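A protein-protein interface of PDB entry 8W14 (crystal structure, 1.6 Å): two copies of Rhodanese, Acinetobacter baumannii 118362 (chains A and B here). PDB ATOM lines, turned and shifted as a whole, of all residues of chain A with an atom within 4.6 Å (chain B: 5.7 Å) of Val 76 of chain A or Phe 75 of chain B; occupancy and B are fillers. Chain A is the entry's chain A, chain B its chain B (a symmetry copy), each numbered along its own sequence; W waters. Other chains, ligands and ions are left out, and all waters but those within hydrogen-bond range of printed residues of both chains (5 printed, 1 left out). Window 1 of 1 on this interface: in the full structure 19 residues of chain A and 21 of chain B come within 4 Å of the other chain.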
ATOM      1  N   ARG A  68      26.606  15.159  -4.957  1.00  0.00           N
ATOM      2  CA  ARG A  68      25.779  15.492  -3.807  1.00  0.00           C
ATOM      3  C   ARG A  68      26.445  15.069  -2.498  1.00  0.00           C
ATOM      4  O   ARG A  68      27.507  14.445  -2.471  1.00  0.00           O
ATOM      5  CB  ARG A  68      24.407  14.831  -3.917  1.00  0.00           C
ATOM      6  CG  ARG A  68      23.608  15.315  -5.118  1.00  0.00           C
ATOM      7  CD  ARG A  68      22.297  14.554  -5.267  1.00  0.00           C
ATOM      8  NE  ARG A  68      22.554  13.127  -5.424  1.00  0.00           N
ATOM      9  CZ  ARG A  68      21.777  12.159  -4.954  1.00  0.00           C
ATOM     10  NH1 ARG A  68      20.632  12.424  -4.341  1.00  0.00           N
ATOM     11  NH2 ARG A  68      22.161  10.894  -5.095  1.00  0.00           N
ATOM     12  N   THR A  69      25.797  15.438  -1.395  1.00  0.00           N
ATOM     13  CA  THR A  69      26.252  15.027  -0.076  1.00  0.00           C
ATOM     14  C   THR A  69      26.005  13.541   0.149  1.00  0.00           C
ATOM     15  O   THR A  69      25.150  12.914  -0.492  1.00  0.00           O
ATOM     16  CB  THR A  69      25.519  15.790   1.033  1.00  0.00           C
ATOM     17  OG1 THR A  69      24.123  15.457   1.013  1.00  0.00           O
ATOM     18  CG2 THR A  69      25.693  17.299   0.900  1.00  0.00           C
ATOM     19  N   GLU A  71      24.612  12.559   2.778  1.00  0.00           N
ATOM     20  CA  GLU A  71      23.275  12.562   3.365  1.00  0.00           C
ATOM     21  C   GLU A  71      22.199  12.404   2.298  1.00  0.00           C
ATOM     22  O   GLU A  71      21.195  11.711   2.508  1.00  0.00           O
ATOM     23  CB  GLU A  71      23.061  13.863   4.141  1.00  0.00           C
ATOM     24  CG  GLU A  71      23.856  13.967   5.437  1.00  0.00           C
ATOM     25  CD  GLU A  71      25.316  14.396   5.275  1.00  0.00           C
ATOM     26  OE1 GLU A  71      25.770  14.693   4.147  1.00  0.00           O
ATOM     27  OE2 GLU A  71      26.013  14.466   6.312  1.00  0.00           O
ATOM     28  N   GLU A  72      22.375  13.067   1.159  1.00  0.00           N
ATOM     29  CA  GLU A  72      21.414  12.909   0.071  1.00  0.00           C
ATOM     30  C   GLU A  72      21.448  11.503  -0.508  1.00  0.00           C
ATOM     31  O   GLU A  72      20.398  10.916  -0.784  1.00  0.00           O
ATOM     32  CB  GLU A  72      21.697  13.933  -1.022  1.00  0.00           C
ATOM     33  CG  GLU A  72      21.272  15.342  -0.661  1.00  0.00           C
ATOM     34  CD  GLU A  72      21.945  16.370  -1.540  1.00  0.00           C
ATOM     35  OE1 GLU A  72      23.119  16.710  -1.257  1.00  0.00           O
ATOM     36  OE2 GLU A  72      21.308  16.819  -2.524  1.00  0.00           O
ATOM     37  N   ARG A  73      22.638  10.946  -0.735  1.00  0.00           N
ATOM     38  CA  ARG A  73      22.687   9.589  -1.266  1.00  0.00           C
ATOM     39  C   ARG A  73      22.024   8.613  -0.307  1.00  0.00           C
ATOM     40  O   ARG A  73      21.322   7.689  -0.737  1.00  0.00           O
ATOM     41  CB  ARG A  73      24.130   9.168  -1.552  1.00  0.00           C
ATOM     42  CG  ARG A  73      24.718   9.839  -2.782  1.00  0.00           C
ATOM     43  CD  ARG A  73      26.218   9.555  -2.906  1.00  0.00           C
ATOM     44  NE  ARG A  73      26.532   8.129  -3.021  1.00  0.00           N
ATOM     45  CZ  ARG A  73      26.561   7.444  -4.161  1.00  0.00           C
ATOM     46  NH1 ARG A  73      26.243   8.002  -5.318  1.00  0.00           N
ATOM     47  NH2 ARG A  73      26.959   6.173  -4.145  1.00  0.00           N
ATOM     48  N   LYS A  74      22.202   8.835   1.003  1.00  0.00           N
ATOM     49  CA  LYS A  74      21.668   7.927   2.011  1.00  0.00           C
ATOM     50  C   LYS A  74      20.153   8.025   2.112  1.00  0.00           C
ATOM     51  O   LYS A  74      19.471   7.004   2.222  1.00  0.00           O
ATOM     52  CB  LYS A  74      22.308   8.229   3.370  1.00  0.00           C
ATOM     53  CG  LYS A  74      21.772   7.391   4.529  1.00  0.00           C
ATOM     54  CD  LYS A  74      22.114   5.922   4.334  1.00  0.00           C
ATOM     55  CE  LYS A  74      21.803   5.107   5.580  1.00  0.00           C
ATOM     56  NZ  LYS A  74      22.195   3.683   5.384  1.00  0.00           N
ATOM     57  N   PHE A  75      19.602   9.237   2.086  1.00  0.00           N
ATOM     58  CA  PHE A  75      18.186   9.403   2.400  1.00  0.00           C
ATOM     59  C   PHE A  75      17.309   9.750   1.209  1.00  0.00           C
ATOM     60  O   PHE A  75      16.112   9.429   1.233  1.00  0.00           O
ATOM     61  CB  PHE A  75      18.014  10.471   3.484  1.00  0.00           C
ATOM     62  CG  PHE A  75      18.530  10.036   4.827  1.00  0.00           C
ATOM     63  CD1 PHE A  75      17.948   8.962   5.486  1.00  0.00           C
ATOM     64  CD2 PHE A  75      19.591  10.696   5.428  1.00  0.00           C
ATOM     65  CE1 PHE A  75      18.413   8.553   6.733  1.00  0.00           C
ATOM     66  CE2 PHE A  75      20.065  10.297   6.674  1.00  0.00           C
ATOM     67  CZ  PHE A  75      19.476   9.214   7.327  1.00  0.00           C
ATOM     68  N   VAL A  76      17.860  10.376   0.175  1.00  0.00           N
ATOM     69  CA  VAL A  76      17.075  10.651  -1.025  1.00  0.00           C
ATOM     70  C   VAL A  76      17.168   9.495  -2.008  1.00  0.00           C
ATOM     71  O   VAL A  76      16.161   9.072  -2.580  1.00  0.00           O
ATOM     72  CB  VAL A  76      17.529  11.968  -1.679  1.00  0.00           C
ATOM     73  CG1 VAL A  76      16.731  12.226  -2.938  1.00  0.00           C
ATOM     74  CG2 VAL A  76      17.377  13.141  -0.719  1.00  0.00           C
ATOM     75  N   GLY A  77      18.356   8.942  -2.173  1.00  0.00           N
ATOM     76  CA  GLY A  77      18.607   7.871  -3.112  1.00  0.00           C
ATOM     77  C   GLY A  77      19.756   8.225  -4.021  1.00  0.00           C
ATOM     78  O   GLY A  77      20.325   9.314  -3.951  1.00  0.00           O
ATOM     79  N   GLY A  90      27.345  17.556   4.251  1.00  0.00           N
ATOM     80  CA  GLY A  90      26.532  17.892   5.399  1.00  0.00           C
ATOM     81  C   GLY A  90      25.287  18.694   5.067  1.00  0.00           C
ATOM     82  O   GLY A  90      25.072  19.165   3.947  1.00  0.00           O
ATOM     83  N   THR A  91      24.445  18.845   6.089  1.00  0.00           N
ATOM     84  CA  THR A  91      23.228  19.640   5.979  1.00  0.00           C
ATOM     85  C   THR A  91      23.502  21.132   5.810  1.00  0.00           C
ATOM     86  O   THR A  91      22.559  21.879   5.530  1.00  0.00           O
ATOM     87  CB  THR A  91      22.316  19.382   7.186  1.00  0.00           C
ATOM     88  OG1 THR A  91      23.027  19.612   8.410  1.00  0.00           O
ATOM     89  CG2 THR A  91      21.806  17.950   7.173  1.00  0.00           C
ATOM     90  N   PHE A  93      26.063  22.171   3.719  1.00  0.00           N
ATOM     91  CA  PHE A  93      26.758  22.284   2.437  1.00  0.00           C
ATOM     92  C   PHE A  93      28.157  22.879   2.611  1.00  0.00           C
ATOM     93  O   PHE A  93      28.542  23.819   1.912  1.00  0.00           O
ATOM     94  CB  PHE A  93      25.940  23.130   1.460  1.00  0.00           C
ATOM     95  CG  PHE A  93      24.552  22.601   1.209  1.00  0.00           C
ATOM     96  CD1 PHE A  93      24.326  21.518   0.378  1.00  0.00           C
ATOM     97  CD2 PHE A  93      23.464  23.214   1.821  1.00  0.00           C
ATOM     98  CE1 PHE A  93      23.026  21.055   0.157  1.00  0.00           C
ATOM     99  CE2 PHE A  93      22.166  22.760   1.613  1.00  0.00           C
ATOM    100  CZ  PHE A  93      21.949  21.676   0.773  1.00  0.00           C
ATOM    101  N   ARG A 118      21.667  17.537  -7.208  1.00  0.00           N
ATOM    102  CA  ARG A 118      20.233  17.531  -6.930  1.00  0.00           C
ATOM    103  C   ARG A 118      19.467  18.297  -7.997  1.00  0.00           C
ATOM    104  O   ARG A 118      18.401  17.860  -8.446  1.00  0.00           O
ATOM    105  CB  ARG A 118      19.976  18.152  -5.554  1.00  0.00           C
ATOM    106  CG  ARG A 118      18.509  18.330  -5.216  1.00  0.00           C
ATOM    107  CD  ARG A 118      18.323  18.712  -3.750  1.00  0.00           C
ATOM    108  NE  ARG A 118      18.871  20.022  -3.428  1.00  0.00           N
ATOM    109  CZ  ARG A 118      18.791  20.574  -2.222  1.00  0.00           C
ATOM    110  NH1 ARG A 118      18.179  19.959  -1.226  1.00  0.00           N
ATOM    111  NH2 ARG A 118      19.332  21.772  -2.013  1.00  0.00           N
ATOM    112  N   PHE A 145      19.254  15.136 -10.087  1.00  0.00           N
ATOM    113  CA  PHE A 145      18.511  13.942  -9.611  1.00  0.00           C
ATOM    114  C   PHE A 145      17.058  14.262  -9.234  1.00  0.00           C
ATOM    115  O   PHE A 145      16.177  13.454  -9.558  1.00  0.00           O
ATOM    116  CB  PHE A 145      19.257  13.365  -8.405  1.00  0.00           C
ATOM    117  CG  PHE A 145      18.840  11.986  -7.967  1.00  0.00           C
ATOM    118  CD1 PHE A 145      18.974  10.900  -8.816  1.00  0.00           C
ATOM    119  CD2 PHE A 145      18.334  11.772  -6.696  1.00  0.00           C
ATOM    120  CE1 PHE A 145      18.598   9.631  -8.405  1.00  0.00           C
ATOM    121  CE2 PHE A 145      17.959  10.503  -6.285  1.00  0.00           C
ATOM    122  CZ  PHE A 145      18.092   9.436  -7.142  1.00  0.00           C
ATOM    123  N   GLU A 146      16.827  15.383  -8.541  1.00  0.00           N
ATOM    124  CA  GLU A 146      15.456  15.678  -8.036  1.00  0.00           C
ATOM    125  C   GLU A 146      14.752  16.791  -8.815  1.00  0.00           C
ATOM    126  O   GLU A 146      13.520  16.891  -8.716  1.00  0.00           O
ATOM    127  CB  GLU A 146      15.529  16.113  -6.575  1.00  0.00           C
ATOM    128  CG  GLU A 146      16.167  15.091  -5.663  1.00  0.00           C
ATOM    129  CD  GLU A 146      15.898  15.394  -4.203  1.00  0.00           C
ATOM    130  OE1 GLU A 146      14.723  15.331  -3.804  1.00  0.00           O
ATOM    131  OE2 GLU A 146      16.857  15.709  -3.479  1.00  0.00           O
ATOM    132  N   ARG A 162      14.555  11.452 -11.351  1.00  0.00           N
ATOM    133  CA  ARG A 162      13.463  10.613 -10.788  1.00  0.00           C
ATOM    134  C   ARG A 162      12.138  10.736 -11.559  1.00  0.00           C
ATOM    135  O   ARG A 162      11.516   9.698 -11.816  1.00  0.00           O
ATOM    136  CB  ARG A 162      13.339  10.880  -9.285  1.00  0.00           C
ATOM    137  CG  ARG A 162      14.659  10.718  -8.547  1.00  0.00           C
ATOM    138  CD  ARG A 162      14.475  10.140  -7.163  1.00  0.00           C
ATOM    139  NE  ARG A 162      13.856  11.099  -6.264  1.00  0.00           N
ATOM    140  CZ  ARG A 162      13.740  10.925  -4.954  1.00  0.00           C
ATOM    141  NH1 ARG A 162      14.205   9.825  -4.388  1.00  0.00           N
ATOM    142  NH2 ARG A 162      13.164  11.853  -4.213  1.00  0.00           N
ATOM    143  N   TRP A 168      17.162   4.364 -10.154  1.00  0.00           N
ATOM    144  CA  TRP A 168      17.705   4.841  -8.885  1.00  0.00           C
ATOM    145  C   TRP A 168      17.187   3.941  -7.771  1.00  0.00           C
ATOM    146  O   TRP A 168      16.216   3.205  -7.954  1.00  0.00           O
ATOM    147  CB  TRP A 168      17.338   6.306  -8.606  1.00  0.00           C
ATOM    148  CG  TRP A 168      15.863   6.536  -8.383  1.00  0.00           C
ATOM    149  CD1 TRP A 168      14.916   6.760  -9.342  1.00  0.00           C
ATOM    150  CD2 TRP A 168      15.169   6.552  -7.123  1.00  0.00           C
ATOM    151  NE1 TRP A 168      13.678   6.925  -8.761  1.00  0.00           N
ATOM    152  CE2 TRP A 168      13.804   6.794  -7.400  1.00  0.00           C
ATOM    153  CE3 TRP A 168      15.567   6.387  -5.791  1.00  0.00           C
ATOM    154  CZ2 TRP A 168      12.834   6.872  -6.394  1.00  0.00           C
ATOM    155  CZ3 TRP A 168      14.597   6.470  -4.787  1.00  0.00           C
ATOM    156  CH2 TRP A 168      13.250   6.709  -5.098  1.00  0.00           C
ATOM    157  N   GLN A 170      17.306   3.433  -3.080  1.00  0.00           N
ATOM    158  CA  GLN A 170      17.642   3.948  -1.757  1.00  0.00           C
ATOM    159  C   GLN A 170      17.549   2.793  -0.766  1.00  0.00           C
ATOM    160  O   GLN A 170      17.282   1.649  -1.142  1.00  0.00           O
ATOM    161  CB  GLN A 170      16.731   5.113  -1.357  1.00  0.00           C
ATOM    162  CG  GLN A 170      15.284   4.697  -1.164  1.00  0.00           C
ATOM    163  CD  GLN A 170      14.378   5.883  -0.922  1.00  0.00           C
ATOM    164  OE1 GLN A 170      13.407   6.078  -1.653  1.00  0.00           O
ATOM    165  NE2 GLN A 170      14.684   6.682   0.101  1.00  0.00           N
ATOM    166  N   ASN B  70      17.668  15.026  11.479  1.00  0.00           N
ATOM    167  CA  ASN B  70      17.728  16.327  10.818  1.00  0.00           C
ATOM    168  C   ASN B  70      18.077  16.174   9.344  1.00  0.00           C
ATOM    169  O   ASN B  70      17.569  16.917   8.494  1.00  0.00           O
ATOM    170  CB  ASN B  70      18.755  17.226  11.507  1.00  0.00           C
ATOM    171  CG  ASN B  70      18.797  18.630  10.908  1.00  0.00           C
ATOM    172  OD1 ASN B  70      17.763  19.294  10.779  1.00  0.00           O
ATOM    173  ND2 ASN B  70      19.987  19.078  10.525  1.00  0.00           N
ATOM    174  N   GLU B  71      18.950  15.213   9.027  1.00  0.00           N
ATOM    175  CA  GLU B  71      19.314  14.945   7.638  1.00  0.00           C
ATOM    176  C   GLU B  71      18.087  14.621   6.791  1.00  0.00           C
ATOM    177  O   GLU B  71      17.959  15.106   5.660  1.00  0.00           O
ATOM    178  CB  GLU B  71      20.322  13.793   7.598  1.00  0.00           C
ATOM    179  CG  GLU B  71      21.720  14.179   8.082  1.00  0.00           C
ATOM    180  CD  GLU B  71      21.891  14.229   9.594  1.00  0.00           C
ATOM    181  OE1 GLU B  71      20.955  13.883  10.341  1.00  0.00           O
ATOM    182  OE2 GLU B  71      22.989  14.638  10.033  1.00  0.00           O
ATOM    183  N   GLU B  72      17.175  13.801   7.319  1.00  0.00           N
ATOM    184  CA  GLU B  72      15.940  13.498   6.598  1.00  0.00           C
ATOM    185  C   GLU B  72      15.046  14.722   6.466  1.00  0.00           C
ATOM    186  O   GLU B  72      14.480  14.973   5.394  1.00  0.00           O
ATOM    187  CB  GLU B  72      15.183  12.375   7.306  1.00  0.00           C
ATOM    188  CG  GLU B  72      15.799  11.021   7.099  1.00  0.00           C
ATOM    189  CD  GLU B  72      15.308  10.022   8.113  1.00  0.00           C
ATOM    190  OE1 GLU B  72      15.833  10.027   9.249  1.00  0.00           O
ATOM    191  OE2 GLU B  72      14.387   9.245   7.785  1.00  0.00           O
ATOM    192  N   ARG B  73      14.880  15.485   7.543  1.00  0.00           N
ATOM    193  CA  ARG B  73      14.054  16.681   7.446  1.00  0.00           C
ATOM    194  C   ARG B  73      14.618  17.662   6.422  1.00  0.00           C
ATOM    195  O   ARG B  73      13.858  18.296   5.680  1.00  0.00           O
ATOM    196  CB  ARG B  73      13.921  17.330   8.827  1.00  0.00           C
ATOM    197  CG  ARG B  73      12.988  16.538   9.756  1.00  0.00           C
ATOM    198  CD  ARG B  73      13.061  17.007  11.206  1.00  0.00           C
ATOM    199  NE  ARG B  73      12.702  18.413  11.365  1.00  0.00           N
ATOM    200  CZ  ARG B  73      11.464  18.872  11.514  1.00  0.00           C
ATOM    201  NH1 ARG B  73      10.411  18.064  11.488  1.00  0.00           N
ATOM    202  NH2 ARG B  73      11.275  20.181  11.681  1.00  0.00           N
ATOM    203  N   LYS B  74      15.953  17.778   6.353  1.00  0.00           N
ATOM    204  CA  LYS B  74      16.597  18.732   5.450  1.00  0.00           C
ATOM    205  C   LYS B  74      16.498  18.292   3.994  1.00  0.00           C
ATOM    206  O   LYS B  74      16.234  19.119   3.113  1.00  0.00           O
ATOM    207  CB  LYS B  74      18.066  18.919   5.850  1.00  0.00           C
ATOM    208  CG  LYS B  74      18.916  19.832   4.940  1.00  0.00           C
ATOM    209  CD  LYS B  74      18.455  21.287   4.965  1.00  0.00           C
ATOM    210  CE  LYS B  74      19.484  22.169   4.231  1.00  0.00           C
ATOM    211  NZ  LYS B  74      19.140  23.621   4.213  1.00  0.00           N
ATOM    212  N   PHE B  75      16.716  17.007   3.716  1.00  0.00           N
ATOM    213  CA  PHE B  75      16.835  16.566   2.333  1.00  0.00           C
ATOM    214  C   PHE B  75      15.640  15.788   1.805  1.00  0.00           C
ATOM    215  O   PHE B  75      15.418  15.795   0.596  1.00  0.00           O
ATOM    216  CB  PHE B  75      18.109  15.731   2.154  1.00  0.00           C
ATOM    217  CG  PHE B  75      19.369  16.542   2.254  1.00  0.00           C
ATOM    218  CD1 PHE B  75      19.650  17.524   1.308  1.00  0.00           C
ATOM    219  CD2 PHE B  75      20.260  16.350   3.299  1.00  0.00           C
ATOM    220  CE1 PHE B  75      20.811  18.290   1.388  1.00  0.00           C
ATOM    221  CE2 PHE B  75      21.439  17.113   3.388  1.00  0.00           C
ATOM    222  CZ  PHE B  75      21.714  18.081   2.432  1.00  0.00           C
ATOM    223  N   VAL B  76      14.868  15.129   2.662  1.00  0.00           N
ATOM    224  CA  VAL B  76      13.650  14.453   2.213  1.00  0.00           C
ATOM    225  C   VAL B  76      12.437  15.360   2.329  1.00  0.00           C
ATOM    226  O   VAL B  76      11.573  15.367   1.447  1.00  0.00           O
ATOM    227  CB  VAL B  76      13.452  13.151   3.009  1.00  0.00           C
ATOM    228  CG1 VAL B  76      12.164  12.438   2.566  1.00  0.00           C
ATOM    229  CG2 VAL B  76      14.649  12.242   2.845  1.00  0.00           C
ATOM    230  N   GLY B  77      12.350  16.121   3.411  1.00  0.00           N
ATOM    231  CA  GLY B  77      11.232  17.000   3.670  1.00  0.00           C
ATOM    232  C   GLY B  77      10.635  16.733   5.031  1.00  0.00           C
ATOM    233  O   GLY B  77      11.063  15.844   5.765  1.00  0.00           O
ATOM    234  N   GLN B 170       9.942  20.909   1.672  1.00  0.00           N
ATOM    235  CA  GLN B 170      11.367  20.672   1.803  1.00  0.00           C
ATOM    236  C   GLN B 170      12.082  21.922   1.338  1.00  0.00           C
ATOM    237  O   GLN B 170      11.471  22.832   0.771  1.00  0.00           O
ATOM    238  CB  GLN B 170      11.823  19.437   1.007  1.00  0.00           C
ATOM    239  CG  GLN B 170      11.671  19.550  -0.520  1.00  0.00           C
ATOM    240  CD  GLN B 170      12.011  18.255  -1.236  1.00  0.00           C
ATOM    241  OE1 GLN B 170      11.209  17.725  -2.011  1.00  0.00           O
ATOM    242  NE2 GLN B 170      13.204  17.730  -0.968  1.00  0.00           N
ATOM    243  N   ASP B 171      13.416  21.898   1.372  1.00  0.00           N
ATOM    244  CA  ASP B 171      14.172  23.041   0.788  1.00  0.00           C
ATOM    245  C   ASP B 171      15.065  22.543  -0.360  1.00  0.00           C
ATOM    246  O   ASP B 171      14.803  21.429  -0.857  1.00  0.00           O
ATOM    247  CB  ASP B 171      14.989  23.789   1.842  1.00  0.00           C
ATOM    248  CG  ASP B 171      16.257  23.056   2.234  1.00  0.00           C
ATOM    249  OD1 ASP B 171      16.161  21.855   2.537  1.00  0.00           O
ATOM    250  OD2 ASP B 171      17.323  23.694   2.223  1.00  0.00           O
HETATM  251  O   HOH W   1      13.984  14.623  -1.468  1.00  0.00           O
HETATM  252  O   HOH W   2      22.463  17.708  10.733  1.00  0.00           O
HETATM  253  O   HOH W   3      18.236  20.951   1.445  1.00  0.00           O
HETATM  254  O   HOH W   4      16.839  17.278  -1.269  1.00  0.00           O
HETATM  255  O   HOH W   5      18.176  23.992  -0.305  1.00  0.00           O
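Among the printed residues, 17 pairs touch across the chains.
Among the printed residues, merely in contact across the chains: Thr 69 of chain A with Phe 75 of chain B, Glu 71 of chain A with Glu 71 of chain B, Glu 71 of chain A with Phe 75 of chain B, Glu 72 of chain A with Phe 75 of chain B, Phe 75 of chain A with Glu 71 of chain B, Phe 75 of chain A with Glu 72 of chain B, Phe 75 of chain A with Val 76 of chain B, Val 76 of chain A with Phe 75 of chain B, Gly 90 of chain A with Phe 75 of chain B, Thr 91 of chain A with Asn 70 of chain B, Thr 91 of chain A with Glu 71 of chain B, Thr 91 of chain A with Lys 74 of chain B, Thr 91 of chain A with Phe 75 of chain B, Phe 93 of chain A with Lys 74 of chain B, Phe 93 of chain A with Phe 75 of chain B, Arg 118 of chain A with Phe 75 of chain B and Arg 118 of chain A with Asp 171 of chain B.
Glu 71 of chain B touches its own counterpart, Glu 71 of chain A. Glu 71 of chain A touches Phe 75 of chain B, and with the chains exchanged Phe 75 of chain A touches Glu 71 of chain B. Glu 72 of chain A touches Phe 75 of chain B, and with the chains exchanged Phe 75 of chain A touches Glu 72 of chain B. Phe 75 of chain A touches Val 76 of chain B, and with the chains exchanged Val 76 of chain A touches Phe 75 of chain B.
NE2 of Gln 170 of chain A lies within hydrogen-bond range of O of Phe 75 of chain A, 3.3 Å away. The backbone NH (N) of Glu 146 of chain A sits at hydrogen-bond distance from the backbone carbonyl oxygen (O) of Arg 118 of chain A (2.9 Å). OG1 of Thr 69 of chain A sits at hydrogen-bond distance from OE1 of Glu 72 of chain A. The backbone carbonyl oxygen (O) of Glu 72 of chain B lies within hydrogen-bond range of the backbone NH (N) of Gly 77 of chain B (3.1 Å). O of Val 76 of chain A sits at hydrogen-bond distance from NH1 of Arg 162 of chain A (2.8 Å). O of Arg 118 of chain A lies within hydrogen-bond range of N of Phe 145 of chain A.
Of the printed residues of chain B, Glu 71 of chain A touches Glu 71 (3.4 Å) and Phe 75 (3.7 Å). Of the printed residues of chain B, Val 76 of chain A touches Phe 75 (3.6 Å). Printed residues of chain B within 4 Å of Arg 118 of chain A: Phe 75 (3.8 Å) and Asp 171 (3.7 Å). Arg 162 of chain A touches none of the printed residues of chain B. Printed residues of chain A within 4 Å of Asn 70 of chain B: Thr 91. Phe 75 of chain B touches just these residues of chain A: Thr 69 (3.8 Å), Glu 71 (3.7 Å), Glu 72 (3.4 Å), Val 76 (3.6 Å), Gly 90 (3.8 Å), Thr 91 (3.9 Å), Phe 93 (3.6 Å) and Arg 118 (3.8 Å). Of the printed residues of chain A, Val 76 of chain B touches Phe 75 (3.6 Å). Gln 170 of chain B touches none of the printed residues of chain A. The nearest residue of chain A that does not touch Phe 75 of chain B is Glu 146 of chain A (4.3 Å). The nearest printed residue of chain B that does not touch Phe 93 of chain A is Asp 171 of chain B (5.0 Å).
Water W3 lies within hydrogen-bond range of OD1 of Asp 171 of chain B (2.5 Å), NH1 of Arg 118 of chain A (2.8 Å) and O of Lys 74 of chain B (3.2 Å). Water W1 lies within hydrogen-bond range of the side-chain carboxylate (OE1) of Glu 146 of chain A (2.6 Å), the backbone carbonyl oxygen (O) of Phe 75 of chain B (2.8 Å) and the side-chain amide nitrogen (NE2) of Gln 170 of chain B (3.2 Å). Water W5 bridges the side-chain carboxylate of Asp 171 of chain B (2.7 Å) and the guanidinium group of Arg 118 of chain A (3.0 Å). Water W4 lies within hydrogen-bond range of the side-chain carboxylate (OE2) of Glu 146 of chain A, the backbone carbonyl oxygen (O) of Phe 75 of chain B and the guanidinium group (NH1) of Arg 118 of chain A. Water W2 lies within hydrogen-bond range of ND2 of Asn 70 of chain B (2.8 Å), OG1 of Thr 91 of chain A (3.1 Å) and OE2 of Glu 71 of chain B (3.2 Å).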
